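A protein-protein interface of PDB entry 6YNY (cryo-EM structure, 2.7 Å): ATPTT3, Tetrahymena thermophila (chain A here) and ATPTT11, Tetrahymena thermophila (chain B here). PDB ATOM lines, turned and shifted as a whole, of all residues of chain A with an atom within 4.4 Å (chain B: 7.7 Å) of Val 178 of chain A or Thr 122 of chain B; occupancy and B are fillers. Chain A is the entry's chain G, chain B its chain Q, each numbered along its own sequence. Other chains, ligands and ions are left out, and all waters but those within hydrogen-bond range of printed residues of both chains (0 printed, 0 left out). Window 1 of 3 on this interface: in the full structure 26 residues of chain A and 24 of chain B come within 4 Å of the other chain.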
ATOM      1  N   ARG A 158      -0.728  -0.365   7.817  1.00  0.00           N
ATOM      2  CA  ARG A 158      -1.001   0.581   8.890  1.00  0.00           C
ATOM      3  C   ARG A 158      -0.029   0.407  10.046  1.00  0.00           C
ATOM      4  O   ARG A 158       0.347   1.390  10.695  1.00  0.00           O
ATOM      5  CB  ARG A 158      -2.441   0.430   9.367  1.00  0.00           C
ATOM      6  CG  ARG A 158      -3.461   0.786   8.307  1.00  0.00           C
ATOM      7  CD  ARG A 158      -4.806   1.103   8.904  1.00  0.00           C
ATOM      8  NE  ARG A 158      -5.751   1.553   7.892  1.00  0.00           N
ATOM      9  CZ  ARG A 158      -6.924   2.111   8.162  1.00  0.00           C
ATOM     10  NH1 ARG A 158      -7.305   2.301   9.416  1.00  0.00           N
ATOM     11  NH2 ARG A 158      -7.717   2.486   7.172  1.00  0.00           N
ATOM     12  N   HIS A 177      -9.109   9.089   8.605  1.00  0.00           N
ATOM     13  CA  HIS A 177     -10.220   8.709   7.749  1.00  0.00           C
ATOM     14  C   HIS A 177      -9.759   8.691   6.301  1.00  0.00           C
ATOM     15  O   HIS A 177      -8.857   9.434   5.907  1.00  0.00           O
ATOM     16  CB  HIS A 177     -11.417   9.654   7.915  1.00  0.00           C
ATOM     17  CG  HIS A 177     -11.140  11.068   7.515  1.00  0.00           C
ATOM     18  ND1 HIS A 177     -11.470  11.568   6.276  1.00  0.00           N
ATOM     19  CD2 HIS A 177     -10.578  12.094   8.195  1.00  0.00           C
ATOM     20  CE1 HIS A 177     -11.117  12.838   6.206  1.00  0.00           C
ATOM     21  NE2 HIS A 177     -10.572  13.181   7.358  1.00  0.00           N
ATOM     22  N   VAL A 178     -10.391   7.830   5.515  1.00  0.00           N
ATOM     23  CA  VAL A 178     -10.006   7.605   4.126  1.00  0.00           C
ATOM     24  C   VAL A 178     -10.855   8.484   3.221  1.00  0.00           C
ATOM     25  O   VAL A 178     -12.088   8.471   3.301  1.00  0.00           O
ATOM     26  CB  VAL A 178     -10.160   6.123   3.751  1.00  0.00           C
ATOM     27  CG1 VAL A 178      -9.798   5.904   2.303  1.00  0.00           C
ATOM     28  CG2 VAL A 178      -9.299   5.263   4.644  1.00  0.00           C
ATOM     29  N   LEU A 179     -10.191   9.241   2.352  1.00  0.00           N
ATOM     30  CA  LEU A 179     -10.868  10.076   1.373  1.00  0.00           C
ATOM     31  C   LEU A 179     -10.928   9.441  -0.007  1.00  0.00           C
ATOM     32  O   LEU A 179     -11.885   9.685  -0.746  1.00  0.00           O
ATOM     33  CB  LEU A 179     -10.170  11.433   1.265  1.00  0.00           C
ATOM     34  CG  LEU A 179     -10.224  12.319   2.508  1.00  0.00           C
ATOM     35  CD1 LEU A 179      -9.313  13.511   2.347  1.00  0.00           C
ATOM     36  CD2 LEU A 179     -11.642  12.773   2.777  1.00  0.00           C
ATOM     37  N   ASP A 180      -9.932   8.638  -0.366  1.00  0.00           N
ATOM     38  CA  ASP A 180      -9.907   7.977  -1.659  1.00  0.00           C
ATOM     39  C   ASP A 180      -8.983   6.775  -1.573  1.00  0.00           C
ATOM     40  O   ASP A 180      -8.059   6.743  -0.757  1.00  0.00           O
ATOM     41  CB  ASP A 180      -9.446   8.926  -2.766  1.00  0.00           C
ATOM     42  CG  ASP A 180      -9.655   8.353  -4.149  1.00  0.00           C
ATOM     43  OD1 ASP A 180     -10.190   7.230  -4.253  1.00  0.00           O
ATOM     44  OD2 ASP A 180      -9.290   9.028  -5.135  1.00  0.00           O
ATOM     45  N   PHE A 217      -3.319   6.295  -1.438  1.00  0.00           N
ATOM     46  CA  PHE A 217      -4.241   6.374  -0.313  1.00  0.00           C
ATOM     47  C   PHE A 217      -4.378   7.831   0.089  1.00  0.00           C
ATOM     48  O   PHE A 217      -3.396   8.453   0.506  1.00  0.00           O
ATOM     49  CB  PHE A 217      -3.740   5.547   0.872  1.00  0.00           C
ATOM     50  CG  PHE A 217      -4.662   4.439   1.279  1.00  0.00           C
ATOM     51  CD1 PHE A 217      -5.952   4.708   1.685  1.00  0.00           C
ATOM     52  CD2 PHE A 217      -4.226   3.129   1.283  1.00  0.00           C
ATOM     53  CE1 PHE A 217      -6.796   3.691   2.064  1.00  0.00           C
ATOM     54  CE2 PHE A 217      -5.065   2.109   1.666  1.00  0.00           C
ATOM     55  CZ  PHE A 217      -6.351   2.390   2.059  1.00  0.00           C
ATOM     56  N   LYS A 218      -5.582   8.378  -0.041  1.00  0.00           N
ATOM     57  CA  LYS A 218      -5.874   9.730   0.419  1.00  0.00           C
ATOM     58  C   LYS A 218      -6.351   9.651   1.863  1.00  0.00           C
ATOM     59  O   LYS A 218      -7.434   9.126   2.139  1.00  0.00           O
ATOM     60  CB  LYS A 218      -6.919  10.399  -0.467  1.00  0.00           C
ATOM     61  CG  LYS A 218      -6.444  10.735  -1.865  1.00  0.00           C
ATOM     62  CD  LYS A 218      -5.365  11.785  -1.846  1.00  0.00           C
ATOM     63  CE  LYS A 218      -5.248  12.468  -3.190  1.00  0.00           C
ATOM     64  NZ  LYS A 218      -5.078  11.495  -4.288  1.00  0.00           N
ATOM     65  N   PHE A 219      -5.545  10.168   2.779  1.00  0.00           N
ATOM     66  CA  PHE A 219      -5.826  10.119   4.203  1.00  0.00           C
ATOM     67  C   PHE A 219      -6.094  11.513   4.750  1.00  0.00           C
ATOM     68  O   PHE A 219      -5.652  12.523   4.198  1.00  0.00           O
ATOM     69  CB  PHE A 219      -4.659   9.488   4.966  1.00  0.00           C
ATOM     70  CG  PHE A 219      -4.601   7.997   4.868  1.00  0.00           C
ATOM     71  CD1 PHE A 219      -5.701   7.225   5.178  1.00  0.00           C
ATOM     72  CD2 PHE A 219      -3.442   7.368   4.467  1.00  0.00           C
ATOM     73  CE1 PHE A 219      -5.645   5.857   5.092  1.00  0.00           C
ATOM     74  CE2 PHE A 219      -3.380   6.001   4.379  1.00  0.00           C
ATOM     75  CZ  PHE A 219      -4.483   5.244   4.689  1.00  0.00           C
ATOM     76  N   ALA B 107     -23.733  12.332  11.972  1.00  0.00           N
ATOM     77  CA  ALA B 107     -23.266  12.230  10.596  1.00  0.00           C
ATOM     78  C   ALA B 107     -24.428  12.019   9.641  1.00  0.00           C
ATOM     79  O   ALA B 107     -24.468  12.614   8.559  1.00  0.00           O
ATOM     80  CB  ALA B 107     -22.258  11.093  10.472  1.00  0.00           C
ATOM     81  N   VAL B 117     -21.848  11.974   1.325  1.00  0.00           N
ATOM     82  CA  VAL B 117     -22.017  10.526   1.394  1.00  0.00           C
ATOM     83  C   VAL B 117     -20.855  10.006   2.232  1.00  0.00           C
ATOM     84  O   VAL B 117     -19.756   9.761   1.726  1.00  0.00           O
ATOM     85  CB  VAL B 117     -22.057   9.873   0.011  1.00  0.00           C
ATOM     86  CG1 VAL B 117     -22.298   8.389   0.134  1.00  0.00           C
ATOM     87  CG2 VAL B 117     -23.133  10.505  -0.838  1.00  0.00           C
ATOM     88  N   ILE B 118     -21.090   9.838   3.526  1.00  0.00           N
ATOM     89  CA  ILE B 118     -20.042   9.483   4.472  1.00  0.00           C
ATOM     90  C   ILE B 118     -19.993   7.970   4.618  1.00  0.00           C
ATOM     91  O   ILE B 118     -21.022   7.325   4.848  1.00  0.00           O
ATOM     92  CB  ILE B 118     -20.279  10.160   5.831  1.00  0.00           C
ATOM     93  CG1 ILE B 118     -20.519  11.654   5.639  1.00  0.00           C
ATOM     94  CG2 ILE B 118     -19.092   9.946   6.739  1.00  0.00           C
ATOM     95  CD1 ILE B 118     -20.790  12.393   6.911  1.00  0.00           C
ATOM     96  N   SER B 119     -18.797   7.406   4.495  1.00  0.00           N
ATOM     97  CA  SER B 119     -18.616   5.975   4.656  1.00  0.00           C
ATOM     98  C   SER B 119     -18.584   5.599   6.132  1.00  0.00           C
ATOM     99  O   SER B 119     -18.312   6.423   7.009  1.00  0.00           O
ATOM    100  CB  SER B 119     -17.329   5.520   3.977  1.00  0.00           C
ATOM    101  OG  SER B 119     -16.211   6.230   4.478  1.00  0.00           O
ATOM    102  N   ALA B 120     -18.867   4.326   6.397  1.00  0.00           N
ATOM    103  CA  ALA B 120     -18.858   3.830   7.766  1.00  0.00           C
ATOM    104  C   ALA B 120     -17.459   3.796   8.356  1.00  0.00           C
ATOM    105  O   ALA B 120     -17.318   3.740   9.581  1.00  0.00           O
ATOM    106  CB  ALA B 120     -19.471   2.435   7.822  1.00  0.00           C
ATOM    107  N   GLU B 121     -16.426   3.827   7.516  1.00  0.00           N
ATOM    108  CA  GLU B 121     -15.057   3.816   8.004  1.00  0.00           C
ATOM    109  C   GLU B 121     -14.636   5.159   8.579  1.00  0.00           C
ATOM    110  O   GLU B 121     -13.635   5.223   9.300  1.00  0.00           O
ATOM    111  CB  GLU B 121     -14.118   3.413   6.868  1.00  0.00           C
ATOM    112  CG  GLU B 121     -12.693   3.134   7.291  1.00  0.00           C
ATOM    113  CD  GLU B 121     -11.855   2.573   6.164  1.00  0.00           C
ATOM    114  OE1 GLU B 121     -12.375   2.462   5.035  1.00  0.00           O
ATOM    115  OE2 GLU B 121     -10.678   2.238   6.407  1.00  0.00           O
ATOM    116  N   THR B 122     -15.374   6.224   8.280  1.00  0.00           N
ATOM    117  CA  THR B 122     -15.058   7.561   8.762  1.00  0.00           C
ATOM    118  C   THR B 122     -15.864   7.966   9.984  1.00  0.00           C
ATOM    119  O   THR B 122     -15.403   8.798  10.769  1.00  0.00           O
ATOM    120  CB  THR B 122     -15.299   8.589   7.653  1.00  0.00           C
ATOM    121  OG1 THR B 122     -14.361   8.388   6.591  1.00  0.00           O
ATOM    122  CG2 THR B 122     -15.168   9.995   8.190  1.00  0.00           C
ATOM    123  N   ILE B 123     -17.052   7.397  10.163  1.00  0.00           N
ATOM    124  CA  ILE B 123     -17.916   7.820  11.263  1.00  0.00           C
ATOM    125  C   ILE B 123     -17.278   7.578  12.626  1.00  0.00           C
ATOM    126  O   ILE B 123     -17.265   8.506  13.450  1.00  0.00           O
ATOM    127  CB  ILE B 123     -19.294   7.147  11.136  1.00  0.00           C
ATOM    128  CG1 ILE B 123     -19.952   7.556   9.819  1.00  0.00           C
ATOM    129  CG2 ILE B 123     -20.156   7.514  12.314  1.00  0.00           C
ATOM    130  CD1 ILE B 123     -21.244   6.863   9.532  1.00  0.00           C
ATOM    131  N   PRO B 124     -16.740   6.394  12.933  1.00  0.00           N
ATOM    132  CA  PRO B 124     -16.310   6.120  14.312  1.00  0.00           C
ATOM    133  C   PRO B 124     -15.148   6.971  14.797  1.00  0.00           C
ATOM    134  O   PRO B 124     -14.760   6.835  15.963  1.00  0.00           O
ATOM    135  CB  PRO B 124     -15.927   4.637  14.264  1.00  0.00           C
ATOM    136  CG  PRO B 124     -15.626   4.364  12.862  1.00  0.00           C
ATOM    137  CD  PRO B 124     -16.522   5.231  12.060  1.00  0.00           C
ATOM    138  N   VAL B 125     -14.573   7.836  13.960  1.00  0.00           N
ATOM    139  CA  VAL B 125     -13.528   8.748  14.405  1.00  0.00           C
ATOM    140  C   VAL B 125     -14.067  10.132  14.718  1.00  0.00           C
ATOM    141  O   VAL B 125     -13.310  10.992  15.187  1.00  0.00           O
ATOM    142  CB  VAL B 125     -12.393   8.849  13.368  1.00  0.00           C
ATOM    143  CG1 VAL B 125     -11.973   7.471  12.901  1.00  0.00           C
ATOM    144  CG2 VAL B 125     -12.809   9.714  12.202  1.00  0.00           C
ATOM    145  N   LEU B 126     -15.351  10.376  14.470  1.00  0.00           N
ATOM    146  CA  LEU B 126     -15.978  11.662  14.766  1.00  0.00           C
ATOM    147  C   LEU B 126     -16.451  11.632  16.213  1.00  0.00           C
ATOM    148  O   LEU B 126     -17.587  11.262  16.512  1.00  0.00           O
ATOM    149  CB  LEU B 126     -17.127  11.927  13.805  1.00  0.00           C
ATOM    150  CG  LEU B 126     -16.797  11.793  12.322  1.00  0.00           C
ATOM    151  CD1 LEU B 126     -18.048  11.912  11.484  1.00  0.00           C
ATOM    152  CD2 LEU B 126     -15.795  12.835  11.915  1.00  0.00           C
ATOM    153  N   ASN B 127     -15.566  12.027  17.125  1.00  0.00           N
ATOM    154  CA  ASN B 127     -15.858  12.020  18.548  1.00  0.00           C
ATOM    155  C   ASN B 127     -15.731  13.391  19.194  1.00  0.00           C
ATOM    156  O   ASN B 127     -15.888  13.499  20.415  1.00  0.00           O
ATOM    157  CB  ASN B 127     -14.937  11.032  19.274  1.00  0.00           C
ATOM    158  CG  ASN B 127     -15.109   9.613  18.788  1.00  0.00           C
ATOM    159  OD1 ASN B 127     -16.065   8.931  19.153  1.00  0.00           O
ATOM    160  ND2 ASN B 127     -14.176   9.155  17.966  1.00  0.00           N
ATOM    161  N   HIS B 131     -13.590  17.529  15.267  1.00  0.00           N
ATOM    162  CA  HIS B 131     -13.461  16.510  14.233  1.00  0.00           C
ATOM    163  C   HIS B 131     -14.448  16.744  13.101  1.00  0.00           C
ATOM    164  O   HIS B 131     -14.105  16.573  11.926  1.00  0.00           O
ATOM    165  CB  HIS B 131     -13.660  15.124  14.839  1.00  0.00           C
ATOM    166  CG  HIS B 131     -12.651  14.773  15.885  1.00  0.00           C
ATOM    167  ND1 HIS B 131     -12.743  13.633  16.653  1.00  0.00           N
ATOM    168  CD2 HIS B 131     -11.525  15.407  16.285  1.00  0.00           C
ATOM    169  CE1 HIS B 131     -11.718  13.583  17.484  1.00  0.00           C
ATOM    170  NE2 HIS B 131     -10.964  14.647  17.281  1.00  0.00           N
ATOM    171  N   TYR B 135     -13.244  17.448   9.197  1.00  0.00           N
ATOM    172  CA  TYR B 135     -13.726  16.529   8.173  1.00  0.00           C
ATOM    173  C   TYR B 135     -14.451  17.279   7.067  1.00  0.00           C
ATOM    174  O   TYR B 135     -14.280  16.973   5.883  1.00  0.00           O
ATOM    175  CB  TYR B 135     -14.645  15.480   8.794  1.00  0.00           C
ATOM    176  CG  TYR B 135     -15.362  14.635   7.770  1.00  0.00           C
ATOM    177  CD1 TYR B 135     -14.681  13.689   7.026  1.00  0.00           C
ATOM    178  CD2 TYR B 135     -16.720  14.789   7.544  1.00  0.00           C
ATOM    179  CE1 TYR B 135     -15.328  12.923   6.087  1.00  0.00           C
ATOM    180  CE2 TYR B 135     -17.374  14.025   6.608  1.00  0.00           C
ATOM    181  CZ  TYR B 135     -16.673  13.092   5.883  1.00  0.00           C
ATOM    182  OH  TYR B 135     -17.317  12.324   4.945  1.00  0.00           O
ATOM    183  N   VAL B 139     -13.389  17.419   3.054  1.00  0.00           N
ATOM    184  CA  VAL B 139     -14.276  17.028   1.968  1.00  0.00           C
ATOM    185  C   VAL B 139     -14.378  18.137   0.934  1.00  0.00           C
ATOM    186  O   VAL B 139     -14.411  17.876  -0.272  1.00  0.00           O
ATOM    187  CB  VAL B 139     -15.657  16.647   2.531  1.00  0.00           C
ATOM    188  CG1 VAL B 139     -16.633  16.366   1.411  1.00  0.00           C
ATOM    189  CG2 VAL B 139     -15.543  15.446   3.434  1.00  0.00           C
ATOM    190  N   PHE B 142     -11.078  18.355  -0.946  1.00  0.00           N
ATOM    191  CA  PHE B 142     -10.929  17.205  -1.828  1.00  0.00           C
ATOM    192  C   PHE B 142     -11.723  17.392  -3.112  1.00  0.00           C
ATOM    193  O   PHE B 142     -11.248  17.051  -4.200  1.00  0.00           O
ATOM    194  CB  PHE B 142     -11.373  15.942  -1.094  1.00  0.00           C
ATOM    195  CG  PHE B 142     -11.113  14.680  -1.848  1.00  0.00           C
ATOM    196  CD1 PHE B 142      -9.890  14.048  -1.753  1.00  0.00           C
ATOM    197  CD2 PHE B 142     -12.087  14.120  -2.647  1.00  0.00           C
ATOM    198  CE1 PHE B 142      -9.646  12.889  -2.440  1.00  0.00           C
ATOM    199  CE2 PHE B 142     -11.844  12.962  -3.338  1.00  0.00           C
ATOM    200  CZ  PHE B 142     -10.624  12.345  -3.234  1.00  0.00           C
ATOM    201  N   PRO B 150     -15.328  12.317  -2.074  1.00  0.00           N
ATOM    202  CA  PRO B 150     -14.536  11.231  -1.494  1.00  0.00           C
ATOM    203  C   PRO B 150     -15.248   9.894  -1.614  1.00  0.00           C
ATOM    204  O   PRO B 150     -16.469   9.812  -1.758  1.00  0.00           O
ATOM    205  CB  PRO B 150     -14.369  11.652  -0.030  1.00  0.00           C
ATOM    206  CG  PRO B 150     -15.437  12.636   0.217  1.00  0.00           C
ATOM    207  CD  PRO B 150     -15.665  13.339  -1.074  1.00  0.00           C
ATOM    208  N   ILE B 151     -14.450   8.828  -1.548  1.00  0.00           N
ATOM    209  CA  ILE B 151     -14.985   7.485  -1.715  1.00  0.00           C
ATOM    210  C   ILE B 151     -15.944   7.174  -0.580  1.00  0.00           C
ATOM    211  O   ILE B 151     -15.654   7.431   0.595  1.00  0.00           O
ATOM    212  CB  ILE B 151     -13.839   6.468  -1.782  1.00  0.00           C
ATOM    213  CG1 ILE B 151     -14.371   5.093  -2.181  1.00  0.00           C
ATOM    214  CG2 ILE B 151     -13.132   6.387  -0.448  1.00  0.00           C
ATOM    215  CD1 ILE B 151     -13.292   4.095  -2.478  1.00  0.00           C
ATOM    216  N   ALA B 152     -17.098   6.615  -0.928  1.00  0.00           N
ATOM    217  CA  ALA B 152     -18.118   6.276   0.053  1.00  0.00           C
ATOM    218  C   ALA B 152     -18.025   4.807   0.450  1.00  0.00           C
ATOM    219  O   ALA B 152     -17.022   4.365   1.009  1.00  0.00           O
ATOM    220  CB  ALA B 152     -19.493   6.584  -0.497  1.00  0.00           C
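Of the printed residues of chain B, His 177 of chain A touches Thr 122 (3.5 Å) and Tyr 135 (3.8 Å). Printed residues of chain B within 4 Å of Val 178 of chain A: Glu 121 and Thr 122. Of the printed residues of chain A, Thr 122 of chain B touches His 177 and Val 178. Of the printed residues of chain A, Tyr 135 of chain B touches His 177. Printed residues of chain A within 4 Å of Phe 142 of chain B: Leu 179 (3.9 Å), Asp 180 (3.6 Å) and Lys 218 (3.9 Å). The nearest printed residue of chain A that does not touch Thr 122 of chain B is Leu 179 of chain A (6.0 Å). The nearest printed residue of chain A that does not touch Glu 121 of chain B is His 177 of chain A (5.1 Å).
Of the 8 printed residues of chain A, 6 touch a printed residue of chain B. Printed residues of chain A that touch a printed residue of chain B: Arg 158, His 177, Val 178, Leu 179, Asp 180 and Lys 218. Hydrophobic or aromatic side chains of chain A that line the printed part of chain B: His 177 and Val 178. Hydrophobic or aromatic side chains of chain B that line the printed part of chain A: Tyr 135, Phe 142, Pro 150 and Ile 151. Among the printed residues, 11 pairs touch across the chains.
NH2 of Arg 158 of chain A is in salt-bridge range of OE2 of Glu 121 of chain B (3.1 Å). N of Ile 151 of chain B lies within hydrogen-bond range of O of Leu 179 of chain A, at 2.8 Å.
N of Leu 179 of chain A sits at hydrogen-bond distance from O of Lys 218 of chain A. The backbone carbonyl oxygen of Asp 180 of chain A lies within hydrogen-bond range of the backbone NH of Lys 218 of chain A, at 3.1 Å.
Thr 122 of chain B touches His 177 of chain A. CE1 of His 177 of chain A touches CD1 of Tyr 135 of chain B (3.8 Å). Glu 121 of chain B touches Val 178 of chain A (OE2 to CG2, 3.8 Å). Thr 122 of chain B touches Val 178 of chain A. Phe 142 of chain B touches Leu 179 of chain A (CZ to O, 3.9 Å). Pro 150 of chain B touches Leu 179 of chain A. Asp 180 of chain A touches Phe 142 of chain B (CB to CZ, 3.6 Å). Asp 180 of chain A touches Ile 151 of chain B (CA to CG2, 3.8 Å). CG of Lys 218 of chain A touches CE1 of Phe 142 of chain B (3.9 Å).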
